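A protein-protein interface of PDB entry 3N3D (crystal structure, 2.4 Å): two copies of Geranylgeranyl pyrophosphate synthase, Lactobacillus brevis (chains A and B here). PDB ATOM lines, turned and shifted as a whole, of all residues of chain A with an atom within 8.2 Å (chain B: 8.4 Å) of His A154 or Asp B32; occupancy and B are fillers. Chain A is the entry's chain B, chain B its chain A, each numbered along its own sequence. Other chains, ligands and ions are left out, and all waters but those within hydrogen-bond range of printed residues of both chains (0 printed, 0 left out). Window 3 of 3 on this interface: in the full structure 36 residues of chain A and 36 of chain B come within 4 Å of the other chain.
The side-chain amide oxygen (OD1) of Asn B33 sits at hydrogen-bond distance from the backbone NH (N) of Ile B36, at 3.1 Å.
Of the 23 printed residues of chain A, 7 touch a printed residue of chain B.
Printed residues of chain B that touch a printed residue of chain A: Gln B30, Leu B31, Asp B32, Asn B33, Ile B36, Asn B112, Tyr B115 and Phe B119.
Hydrophobic or aromatic side chains of chain B within 4 Å of the printed part of chain A: Leu B31, Ile B36, Tyr B115 and Phe B119.
Among the printed residues, pairs that only touch across the chains: Glu A152 with Tyr B115, His A146 with Phe B119, Met A156 with Asn B33, Leu A153 with Tyr B115, Leu A153 with Ile B36, Leu A153 with Asn B112, His A154 with Asp B32 and Gln A150 with Leu B31.
The side-chain amide nitrogen (NE2) of Gln A150 sits at hydrogen-bond distance from the backbone carbonyl oxygen (O) of Gln B30 (3.4 Å).
The side-chain carboxylate (OD1) of Asp B32 lies close to the side-chain amide oxygen (OE1) of Gln A150 (3.2 Å).
The side-chain amide nitrogen of Asn B33 sits at hydrogen-bond distance from the backbone carbonyl oxygen of Leu A153, at 2.9 Å.
The side-chain carboxylate (OD2) of Asp A157 sits at hydrogen-bond distance from the side-chain amide nitrogen (ND2) of Asn B33 (3.4 Å).
SD of Met A156 sits at hydrogen-bond distance from ND2 of Asn B112, at 3.1 Å.
No position is printed for both chains.
Of the 13 pairs that touch across the chains among the printed residues, none has its exchanged pair printed and touching as well.
Of the printed residues of chain B, Glu A152 touches Tyr B115 (3.3 Å).
Of chain B, only Asp B32 (3.9 Å) comes within 4 Å of His A154.
Of the printed residues of chain B, Met A156 touches Asn B33 and Asn B112.
Asp B32 touches just these residues of chain A: Gln A150 (3.2 Å) and His A154 (3.9 Å).
Of the printed residues of chain A, Asn B112 touches Leu A153 (3.9 Å) and Met A156 (3.1 Å).
The nearest residue of chain A that does not touch Asp B32 is Asp A157 (4.7 Å).
The nearest printed residue of chain B that does not touch Glu A152 is Asn B112 (5.5 Å).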
ATOM      1  N   HIS A 146      19.257   1.265   7.708  1.00  0.00           N
ATOM      2  CA  HIS A 146      18.877   2.334   6.784  1.00  0.00           C
ATOM      3  C   HIS A 146      18.003   1.809   5.635  1.00  0.00           C
ATOM      4  O   HIS A 146      16.964   2.399   5.357  1.00  0.00           O
ATOM      5  CB  HIS A 146      20.123   3.062   6.255  1.00  0.00           C
ATOM      6  CG  HIS A 146      19.823   4.281   5.433  1.00  0.00           C
ATOM      7  ND1 HIS A 146      20.015   5.562   5.904  1.00  0.00           N
ATOM      8  CD2 HIS A 146      19.368   4.412   4.163  1.00  0.00           C
ATOM      9  CE1 HIS A 146      19.683   6.429   4.966  1.00  0.00           C
ATOM     10  NE2 HIS A 146      19.284   5.758   3.900  1.00  0.00           N
ATOM     11  N   ARG A 147      18.406   0.712   4.989  1.00  0.00           N
ATOM     12  CA  ARG A 147      17.623   0.145   3.876  1.00  0.00           C
ATOM     13  C   ARG A 147      16.293  -0.463   4.310  1.00  0.00           C
ATOM     14  O   ARG A 147      15.304  -0.372   3.575  1.00  0.00           O
ATOM     15  CB  ARG A 147      18.423  -0.876   3.050  1.00  0.00           C
ATOM     16  CG  ARG A 147      19.142  -0.274   1.836  1.00  0.00           C
ATOM     17  CD  ARG A 147      19.842  -1.324   0.974  1.00  0.00           C
ATOM     18  NE  ARG A 147      20.843  -2.094   1.720  1.00  0.00           N
ATOM     19  CZ  ARG A 147      22.119  -1.741   1.886  1.00  0.00           C
ATOM     20  NH1 ARG A 147      22.929  -2.526   2.585  1.00  0.00           N
ATOM     21  NH2 ARG A 147      22.591  -0.613   1.363  1.00  0.00           N
ATOM     22  N   ILE A 148      16.268  -1.079   5.493  1.00  0.00           N
ATOM     23  CA  ILE A 148      15.030  -1.636   6.036  1.00  0.00           C
ATOM     24  C   ILE A 148      14.026  -0.517   6.321  1.00  0.00           C
ATOM     25  O   ILE A 148      12.856  -0.627   5.969  1.00  0.00           O
ATOM     26  CB  ILE A 148      15.276  -2.501   7.300  1.00  0.00           C
ATOM     27  CG1 ILE A 148      16.121  -3.722   6.952  1.00  0.00           C
ATOM     28  CG2 ILE A 148      13.961  -2.974   7.918  1.00  0.00           C
ATOM     29  CD1 ILE A 148      16.809  -4.341   8.147  1.00  0.00           C
ATOM     30  N   LEU A 149      14.496   0.576   6.910  1.00  0.00           N
ATOM     31  CA  LEU A 149      13.601   1.670   7.268  1.00  0.00           C
ATOM     32  C   LEU A 149      13.246   2.576   6.095  1.00  0.00           C
ATOM     33  O   LEU A 149      12.238   3.279   6.139  1.00  0.00           O
ATOM     34  CB  LEU A 149      14.147   2.447   8.466  1.00  0.00           C
ATOM     35  CG  LEU A 149      14.119   1.592   9.742  1.00  0.00           C
ATOM     36  CD1 LEU A 149      15.009   2.170  10.797  1.00  0.00           C
ATOM     37  CD2 LEU A 149      12.702   1.410  10.285  1.00  0.00           C
ATOM     38  N   GLN A 150      14.076   2.547   5.052  1.00  0.00           N
ATOM     39  CA  GLN A 150      13.747   3.141   3.758  1.00  0.00           C
ATOM     40  C   GLN A 150      12.590   2.376   3.140  1.00  0.00           C
ATOM     41  O   GLN A 150      11.582   2.973   2.767  1.00  0.00           O
ATOM     42  CB  GLN A 150      14.952   3.070   2.814  1.00  0.00           C
ATOM     43  CG  GLN A 150      15.836   4.312   2.784  1.00  0.00           C
ATOM     44  CD  GLN A 150      15.636   5.154   1.529  1.00  0.00           C
ATOM     45  OE1 GLN A 150      14.710   4.923   0.749  1.00  0.00           O
ATOM     46  NE2 GLN A 150      16.514   6.135   1.329  1.00  0.00           N
ATOM     47  N   GLY A 151      12.745   1.053   3.053  1.00  0.00           N
ATOM     48  CA  GLY A 151      11.764   0.161   2.429  1.00  0.00           C
ATOM     49  C   GLY A 151      10.449   0.060   3.183  1.00  0.00           C
ATOM     50  O   GLY A 151       9.401  -0.212   2.587  1.00  0.00           O
ATOM     51  N   GLU A 152      10.511   0.276   4.495  1.00  0.00           N
ATOM     52  CA  GLU A 152       9.325   0.332   5.336  1.00  0.00           C
ATOM     53  C   GLU A 152       8.569   1.638   5.089  1.00  0.00           C
ATOM     54  O   GLU A 152       7.338   1.652   5.082  1.00  0.00           O
ATOM     55  CB  GLU A 152       9.716   0.207   6.807  1.00  0.00           C
ATOM     56  CG  GLU A 152       8.730  -0.576   7.636  1.00  0.00           C
ATOM     57  CD  GLU A 152       8.903  -2.084   7.544  1.00  0.00           C
ATOM     58  OE1 GLU A 152       7.949  -2.768   7.106  1.00  0.00           O
ATOM     59  OE2 GLU A 152       9.984  -2.588   7.922  1.00  0.00           O
ATOM     60  N   LEU A 153       9.315   2.723   4.881  1.00  0.00           N
ATOM     61  CA  LEU A 153       8.743   4.031   4.537  1.00  0.00           C
ATOM     62  C   LEU A 153       8.284   4.113   3.082  1.00  0.00           C
ATOM     63  O   LEU A 153       7.493   4.989   2.728  1.00  0.00           O
ATOM     64  CB  LEU A 153       9.749   5.151   4.812  1.00  0.00           C
ATOM     65  CG  LEU A 153       9.788   5.761   6.215  1.00  0.00           C
ATOM     66  CD1 LEU A 153      11.083   6.525   6.452  1.00  0.00           C
ATOM     67  CD2 LEU A 153       8.587   6.664   6.461  1.00  0.00           C
ATOM     68  N   HIS A 154       8.792   3.209   2.245  1.00  0.00           N
ATOM     69  CA  HIS A 154       8.445   3.179   0.826  1.00  0.00           C
ATOM     70  C   HIS A 154       7.087   2.516   0.585  1.00  0.00           C
ATOM     71  O   HIS A 154       6.444   2.773  -0.434  1.00  0.00           O
ATOM     72  CB  HIS A 154       9.549   2.485   0.016  1.00  0.00           C
ATOM     73  CG  HIS A 154       9.508   2.785  -1.453  1.00  0.00           C
ATOM     74  ND1 HIS A 154       9.641   4.061  -1.958  1.00  0.00           N
ATOM     75  CD2 HIS A 154       9.360   1.969  -2.523  1.00  0.00           C
ATOM     76  CE1 HIS A 154       9.568   4.021  -3.276  1.00  0.00           C
ATOM     77  NE2 HIS A 154       9.398   2.763  -3.645  1.00  0.00           N
ATOM     78  N   GLN A 155       6.659   1.681   1.535  1.00  0.00           N
ATOM     79  CA  GLN A 155       5.350   1.013   1.515  1.00  0.00           C
ATOM     80  C   GLN A 155       4.183   2.004   1.453  1.00  0.00           C
ATOM     81  O   GLN A 155       3.161   1.717   0.827  1.00  0.00           O
ATOM     82  CB  GLN A 155       5.199   0.124   2.753  1.00  0.00           C
ATOM     83  CG  GLN A 155       4.046  -0.884   2.704  1.00  0.00           C
ATOM     84  CD  GLN A 155       4.476  -2.278   2.264  1.00  0.00           C
ATOM     85  OE1 GLN A 155       3.666  -3.050   1.747  1.00  0.00           O
ATOM     86  NE2 GLN A 155       5.747  -2.612   2.479  1.00  0.00           N
ATOM     87  N   MET A 156       4.353   3.158   2.103  1.00  0.00           N
ATOM     88  CA  MET A 156       3.380   4.257   2.079  1.00  0.00           C
ATOM     89  C   MET A 156       3.085   4.740   0.652  1.00  0.00           C
ATOM     90  O   MET A 156       1.926   4.966   0.296  1.00  0.00           O
ATOM     91  CB  MET A 156       3.873   5.429   2.941  1.00  0.00           C
ATOM     92  CG  MET A 156       2.824   6.515   3.202  1.00  0.00           C
ATOM     93  SD  MET A 156       3.494   8.085   3.810  1.00  0.00           S
ATOM     94  CE  MET A 156       3.552   9.049   2.300  1.00  0.00           C
ATOM     95  N   ASP A 157       4.134   4.872  -0.158  1.00  0.00           N
ATOM     96  CA  ASP A 157       4.000   5.322  -1.546  1.00  0.00           C
ATOM     97  C   ASP A 157       3.525   4.226  -2.508  1.00  0.00           C
ATOM     98  O   ASP A 157       3.292   4.494  -3.690  1.00  0.00           O
ATOM     99  CB  ASP A 157       5.317   5.932  -2.046  1.00  0.00           C
ATOM    100  CG  ASP A 157       5.528   7.361  -1.564  1.00  0.00           C
ATOM    101  OD1 ASP A 157       4.563   7.995  -1.082  1.00  0.00           O
ATOM    102  OD2 ASP A 157       6.669   7.856  -1.678  1.00  0.00           O
ATOM    103  N   LEU A 158       3.382   3.002  -2.004  1.00  0.00           N
ATOM    104  CA  LEU A 158       2.917   1.881  -2.822  1.00  0.00           C
ATOM    105  C   LEU A 158       1.496   1.440  -2.461  1.00  0.00           C
ATOM    106  O   LEU A 158       0.943   0.526  -3.081  1.00  0.00           O
ATOM    107  CB  LEU A 158       3.889   0.697  -2.728  1.00  0.00           C
ATOM    108  CG  LEU A 158       5.360   0.892  -3.122  1.00  0.00           C
ATOM    109  CD1 LEU A 158       6.113  -0.421  -2.977  1.00  0.00           C
ATOM    110  CD2 LEU A 158       5.525   1.459  -4.534  1.00  0.00           C
ATOM    111  N   ASN A 159       0.916   2.094  -1.456  1.00  0.00           N
ATOM    112  CA  ASN A 159      -0.466   1.839  -1.062  1.00  0.00           C
ATOM    113  C   ASN A 159      -1.449   2.364  -2.103  1.00  0.00           C
ATOM    114  O   ASN A 159      -1.280   3.476  -2.619  1.00  0.00           O
ATOM    115  CB  ASN A 159      -0.764   2.466   0.301  1.00  0.00           C
ATOM    116  CG  ASN A 159      -0.023   1.788   1.437  1.00  0.00           C
ATOM    117  OD1 ASN A 159       0.470   2.450   2.346  1.00  0.00           O
ATOM    118  ND2 ASN A 159       0.057   0.462   1.394  1.00  0.00           N
ATOM    119  N   ARG A 161      -1.874   1.400  -5.176  1.00  0.00           N
ATOM    120  CA  ARG A 161      -1.291   1.528  -6.504  1.00  0.00           C
ATOM    121  C   ARG A 161      -1.636   0.332  -7.381  1.00  0.00           C
ATOM    122  O   ARG A 161      -1.267  -0.804  -7.080  1.00  0.00           O
ATOM    123  CB  ARG A 161       0.225   1.735  -6.427  1.00  0.00           C
ATOM    124  CG  ARG A 161       0.653   3.149  -6.027  1.00  0.00           C
ATOM    125  CD  ARG A 161       0.158   4.200  -7.021  1.00  0.00           C
ATOM    126  NE  ARG A 161       1.004   5.393  -7.041  1.00  0.00           N
ATOM    127  CZ  ARG A 161       2.044   5.571  -7.855  1.00  0.00           C
ATOM    128  NH1 ARG A 161       2.391   4.634  -8.729  1.00  0.00           N
ATOM    129  NH2 ARG A 161       2.746   6.693  -7.793  1.00  0.00           N
ATOM    130  N   ILE A 164       1.618  -0.446 -10.211  1.00  0.00           N
ATOM    131  CA  ILE A 164       2.932  -0.824  -9.682  1.00  0.00           C
ATOM    132  C   ILE A 164       3.580  -1.947 -10.506  1.00  0.00           C
ATOM    133  O   ILE A 164       2.953  -2.973 -10.787  1.00  0.00           O
ATOM    134  CB  ILE A 164       2.864  -1.162  -8.150  1.00  0.00           C
ATOM    135  CG1 ILE A 164       4.220  -1.639  -7.615  1.00  0.00           C
ATOM    136  CG2 ILE A 164       1.750  -2.165  -7.851  1.00  0.00           C
ATOM    137  CD1 ILE A 164       4.268  -1.851  -6.112  1.00  0.00           C
ATOM    138  N   ASP A 167       9.131  -4.825 -10.657  1.00  0.00           N
ATOM    139  CA  ASP A 167      10.427  -4.367 -10.166  1.00  0.00           C
ATOM    140  C   ASP A 167      10.326  -3.605  -8.841  1.00  0.00           C
ATOM    141  O   ASP A 167      11.214  -3.709  -7.991  1.00  0.00           O
ATOM    142  CB  ASP A 167      11.094  -3.488 -11.226  1.00  0.00           C
ATOM    143  CG  ASP A 167      12.606  -3.579 -11.193  1.00  0.00           C
ATOM    144  OD1 ASP A 167      13.218  -3.155 -10.189  1.00  0.00           O
ATOM    145  OD2 ASP A 167      13.186  -4.070 -12.185  1.00  0.00           O
ATOM    146  N   ALA A 168       9.246  -2.843  -8.677  1.00  0.00           N
ATOM    147  CA  ALA A 168       9.011  -2.075  -7.453  1.00  0.00           C
ATOM    148  C   ALA A 168       8.600  -2.974  -6.290  1.00  0.00           C
ATOM    149  O   ALA A 168       8.898  -2.665  -5.132  1.00  0.00           O
ATOM    150  CB  ALA A 168       7.970  -0.994  -7.689  1.00  0.00           C
ATOM    151  N   TYR A 169       7.913  -4.073  -6.608  1.00  0.00           N
ATOM    152  CA  TYR A 169       7.575  -5.108  -5.630  1.00  0.00           C
ATOM    153  C   TYR A 169       8.843  -5.782  -5.119  1.00  0.00           C
ATOM    154  O   TYR A 169       8.979  -6.033  -3.918  1.00  0.00           O
ATOM    155  CB  TYR A 169       6.626  -6.157  -6.230  1.00  0.00           C
ATOM    156  CG  TYR A 169       6.394  -7.366  -5.337  1.00  0.00           C
ATOM    157  CD1 TYR A 169       5.444  -7.331  -4.316  1.00  0.00           C
ATOM    158  CD2 TYR A 169       7.131  -8.544  -5.513  1.00  0.00           C
ATOM    159  CE1 TYR A 169       5.232  -8.437  -3.491  1.00  0.00           C
ATOM    160  CE2 TYR A 169       6.932  -9.649  -4.694  1.00  0.00           C
ATOM    161  CZ  TYR A 169       5.983  -9.591  -3.687  1.00  0.00           C
ATOM    162  OH  TYR A 169       5.787 -10.687  -2.876  1.00  0.00           O
ATOM    163  N   ASN A 171      11.884  -4.522  -5.106  1.00  0.00           N
ATOM    164  CA  ASN A 171      12.573  -3.524  -4.292  1.00  0.00           C
ATOM    165  C   ASN A 171      11.985  -3.389  -2.898  1.00  0.00           C
ATOM    166  O   ASN A 171      12.729  -3.298  -1.921  1.00  0.00           O
ATOM    167  CB  ASN A 171      12.558  -2.159  -4.983  1.00  0.00           C
ATOM    168  CG  ASN A 171      13.807  -1.908  -5.803  1.00  0.00           C
ATOM    169  OD1 ASN A 171      14.139  -2.673  -6.713  1.00  0.00           O
ATOM    170  ND2 ASN A 171      14.510  -0.825  -5.485  1.00  0.00           N
ATOM    171  N   GLU A 172      10.652  -3.368  -2.825  1.00  0.00           N
ATOM    172  CA  GLU A 172       9.925  -3.249  -1.564  1.00  0.00           C
ATOM    173  C   GLU A 172      10.281  -4.392  -0.628  1.00  0.00           C
ATOM    174  O   GLU A 172      10.670  -4.160   0.518  1.00  0.00           O
ATOM    175  CB  GLU A 172       8.413  -3.237  -1.804  1.00  0.00           C
ATOM    176  CG  GLU A 172       7.588  -3.056  -0.528  1.00  0.00           C
ATOM    177  CD  GLU A 172       6.393  -4.003  -0.446  1.00  0.00           C
ATOM    178  OE1 GLU A 172       6.275  -4.719   0.573  1.00  0.00           O
ATOM    179  OE2 GLU A 172       5.575  -4.038  -1.393  1.00  0.00           O
ATOM    180  N   ILE A 173      10.175  -5.620  -1.130  1.00  0.00           N
ATOM    181  CA  ILE A 173      10.416  -6.797  -0.304  1.00  0.00           C
ATOM    182  C   ILE A 173      11.905  -7.055  -0.033  1.00  0.00           C
ATOM    183  O   ILE A 173      12.246  -7.817   0.880  1.00  0.00           O
ATOM    184  CB  ILE A 173       9.692  -8.064  -0.847  1.00  0.00           C
ATOM    185  CG1 ILE A 173      10.341  -8.580  -2.136  1.00  0.00           C
ATOM    186  CG2 ILE A 173       8.200  -7.786  -1.040  1.00  0.00           C
ATOM    187  CD1 ILE A 173       9.965 -10.021  -2.479  1.00  0.00           C
ATOM    188  N   GLY A 175      14.048  -4.556   0.877  1.00  0.00           N
ATOM    189  CA  GLY A 175      14.248  -3.787   2.099  1.00  0.00           C
ATOM    190  C   GLY A 175      13.545  -4.400   3.297  1.00  0.00           C
ATOM    191  O   GLY A 175      14.167  -4.639   4.333  1.00  0.00           O
ATOM    192  N   VAL B  29      19.829  14.025   5.309  1.00  0.00           N
ATOM    193  CA  VAL B  29      18.549  13.344   5.210  1.00  0.00           C
ATOM    194  C   VAL B  29      18.197  13.150   3.738  1.00  0.00           C
ATOM    195  O   VAL B  29      17.732  14.079   3.067  1.00  0.00           O
ATOM    196  CB  VAL B  29      17.432  14.127   5.926  1.00  0.00           C
ATOM    197  CG1 VAL B  29      16.127  13.344   5.886  1.00  0.00           C
ATOM    198  CG2 VAL B  29      17.822  14.436   7.365  1.00  0.00           C
ATOM    199  N   GLN B  30      18.450  11.945   3.235  1.00  0.00           N
ATOM    200  CA  GLN B  30      18.109  11.596   1.855  1.00  0.00           C
ATOM    201  C   GLN B  30      17.169  10.396   1.823  1.00  0.00           C
ATOM    202  O   GLN B  30      17.509   9.298   2.272  1.00  0.00           O
ATOM    203  CB  GLN B  30      19.360  11.378   0.989  1.00  0.00           C
ATOM    204  CG  GLN B  30      20.518  10.640   1.673  1.00  0.00           C
ATOM    205  CD  GLN B  30      21.777  10.564   0.814  1.00  0.00           C
ATOM    206  OE1 GLN B  30      21.756  10.880  -0.379  1.00  0.00           O
ATOM    207  NE2 GLN B  30      22.879  10.138   1.423  1.00  0.00           N
ATOM    208  N   LEU B  31      15.978  10.633   1.286  1.00  0.00           N
ATOM    209  CA  LEU B  31      14.865   9.707   1.417  1.00  0.00           C
ATOM    210  C   LEU B  31      14.100   9.563   0.102  1.00  0.00           C
ATOM    211  O   LEU B  31      13.914  10.545  -0.626  1.00  0.00           O
ATOM    212  CB  LEU B  31      13.939  10.216   2.525  1.00  0.00           C
ATOM    213  CG  LEU B  31      13.062   9.278   3.354  1.00  0.00           C
ATOM    214  CD1 LEU B  31      13.696   7.909   3.566  1.00  0.00           C
ATOM    215  CD2 LEU B  31      12.821   9.944   4.688  1.00  0.00           C
ATOM    216  N   ASP B  32      13.677   8.331  -0.195  1.00  0.00           N
ATOM    217  CA  ASP B  32      12.886   8.018  -1.394  1.00  0.00           C
ATOM    218  C   ASP B  32      11.517   8.689  -1.341  1.00  0.00           C
ATOM    219  O   ASP B  32      11.105   9.370  -2.288  1.00  0.00           O
ATOM    220  CB  ASP B  32      12.700   6.499  -1.543  1.00  0.00           C
ATOM    221  CG  ASP B  32      13.866   5.822  -2.249  1.00  0.00           C
ATOM    222  OD1 ASP B  32      15.017   6.293  -2.116  1.00  0.00           O
ATOM    223  OD2 ASP B  32      13.628   4.804  -2.933  1.00  0.00           O
ATOM    224  N   ASN B  33      10.834   8.480  -0.218  1.00  0.00           N
ATOM    225  CA  ASN B  33       9.533   9.061   0.074  1.00  0.00           C
ATOM    226  C   ASN B  33       9.647  10.583   0.229  1.00  0.00           C
ATOM    227  O   ASN B  33       9.924  11.075   1.320  1.00  0.00           O
ATOM    228  CB  ASN B  33       8.998   8.407   1.353  1.00  0.00           C
ATOM    229  CG  ASN B  33       7.532   8.702   1.615  1.00  0.00           C
ATOM    230  OD1 ASN B  33       7.121   9.856   1.738  1.00  0.00           O
ATOM    231  ND2 ASN B  33       6.739   7.643   1.742  1.00  0.00           N
ATOM    232  N   GLN B  34       9.438  11.316  -0.865  1.00  0.00           N
ATOM    233  CA  GLN B  34       9.586  12.782  -0.859  1.00  0.00           C
ATOM    234  C   GLN B  34       8.587  13.570   0.022  1.00  0.00           C
ATOM    235  O   GLN B  34       8.961  14.624   0.547  1.00  0.00           O
ATOM    236  CB  GLN B  34       9.738  13.367  -2.293  1.00  0.00           C
ATOM    237  CG  GLN B  34       8.496  14.016  -2.955  1.00  0.00           C
ATOM    238  CD  GLN B  34       8.225  15.453  -2.486  1.00  0.00           C
ATOM    239  OE1 GLN B  34       7.162  15.748  -1.934  1.00  0.00           O
ATOM    240  NE2 GLN B  34       9.195  16.340  -2.690  1.00  0.00           N
ATOM    241  N   PRO B  35       7.323  13.092   0.170  1.00  0.00           N
ATOM    242  CA  PRO B  35       6.443  13.815   1.096  1.00  0.00           C
ATOM    243  C   PRO B  35       6.907  13.788   2.553  1.00  0.00           C
ATOM    244  O   PRO B  35       6.752  14.780   3.266  1.00  0.00           O
ATOM    245  CB  PRO B  35       5.113  13.071   0.951  1.00  0.00           C
ATOM    246  CG  PRO B  35       5.133  12.554  -0.434  1.00  0.00           C
ATOM    247  CD  PRO B  35       6.549  12.122  -0.638  1.00  0.00           C
ATOM    248  N   ILE B  36       7.483  12.666   2.973  1.00  0.00           N
ATOM    249  CA  ILE B  36       7.966  12.497   4.341  1.00  0.00           C
ATOM    250  C   ILE B  36       9.357  13.132   4.526  1.00  0.00           C
ATOM    251  O   ILE B  36       9.733  13.527   5.632  1.00  0.00           O
ATOM    252  CB  ILE B  36       7.906  10.998   4.755  1.00  0.00           C
ATOM    253  CG1 ILE B  36       7.462  10.841   6.196  1.00  0.00           C
ATOM    254  CG2 ILE B  36       9.214  10.279   4.524  1.00  0.00           C
ATOM    255  CD1 ILE B  36       6.447   9.751   6.365  1.00  0.00           C
ATOM    256  N   HIS B  37      10.092  13.243   3.420  1.00  0.00           N
ATOM    257  CA  HIS B  37      11.400  13.889   3.366  1.00  0.00           C
ATOM    258  C   HIS B  37      11.252  15.402   3.524  1.00  0.00           C
ATOM    259  O   HIS B  37      12.062  16.044   4.196  1.00  0.00           O
ATOM    260  CB  HIS B  37      12.082  13.540   2.035  1.00  0.00           C
ATOM    261  CG  HIS B  37      13.339  14.306   1.763  1.00  0.00           C
ATOM    262  ND1 HIS B  37      13.364  15.442   0.982  1.00  0.00           N
ATOM    263  CD2 HIS B  37      14.620  14.083   2.144  1.00  0.00           C
ATOM    264  CE1 HIS B  37      14.602  15.895   0.907  1.00  0.00           C
ATOM    265  NE2 HIS B  37      15.383  15.088   1.603  1.00  0.00           N
ATOM    266  N   ASN B 112       3.975   6.107  10.108  1.00  0.00           N
ATOM    267  CA  ASN B 112       4.919   6.819   9.266  1.00  0.00           C
ATOM    268  C   ASN B 112       5.795   7.796  10.056  1.00  0.00           C
ATOM    269  O   ASN B 112       6.988   7.937   9.771  1.00  0.00           O
ATOM    270  CB  ASN B 112       4.172   7.524   8.140  1.00  0.00           C
ATOM    271  CG  ASN B 112       3.426   6.549   7.233  1.00  0.00           C
ATOM    272  OD1 ASN B 112       3.768   5.366   7.144  1.00  0.00           O
ATOM    273  ND2 ASN B 112       2.399   7.047   6.559  1.00  0.00           N
ATOM    274  N   TYR B 115       8.271   5.548  11.884  1.00  0.00           N
ATOM    275  CA  TYR B 115       9.274   5.146  10.899  1.00  0.00           C
ATOM    276  C   TYR B 115      10.252   6.273  10.578  1.00  0.00           C
ATOM    277  O   TYR B 115      11.456   6.028  10.488  1.00  0.00           O
ATOM    278  CB  TYR B 115       8.624   4.637   9.603  1.00  0.00           C
ATOM    279  CG  TYR B 115       7.950   3.284   9.701  1.00  0.00           C
ATOM    280  CD1 TYR B 115       6.864   2.969   8.876  1.00  0.00           C
ATOM    281  CD2 TYR B 115       8.387   2.320  10.617  1.00  0.00           C
ATOM    282  CE1 TYR B 115       6.234   1.729   8.959  1.00  0.00           C
ATOM    283  CE2 TYR B 115       7.761   1.075  10.715  1.00  0.00           C
ATOM    284  CZ  TYR B 115       6.683   0.792   9.888  1.00  0.00           C
ATOM    285  OH  TYR B 115       6.070  -0.435   9.973  1.00  0.00           O
ATOM    286  N   PHE B 119      14.150   6.221  11.185  1.00  0.00           N
ATOM    287  CA  PHE B 119      15.040   6.625  10.118  1.00  0.00           C
ATOM    288  C   PHE B 119      16.105   7.600  10.607  1.00  0.00           C
ATOM    289  O   PHE B 119      17.285   7.441  10.287  1.00  0.00           O
ATOM    290  CB  PHE B 119      14.231   7.248   8.972  1.00  0.00           C
ATOM    291  CG  PHE B 119      15.073   7.852   7.881  1.00  0.00           C
ATOM    292  CD1 PHE B 119      15.765   7.040   6.982  1.00  0.00           C
ATOM    293  CD2 PHE B 119      15.157   9.234   7.734  1.00  0.00           C
ATOM    294  CE1 PHE B 119      16.543   7.597   5.969  1.00  0.00           C
ATOM    295  CE2 PHE B 119      15.938   9.800   6.720  1.00  0.00           C
ATOM    296  CZ  PHE B 119      16.631   8.983   5.840  1.00  0.00           C
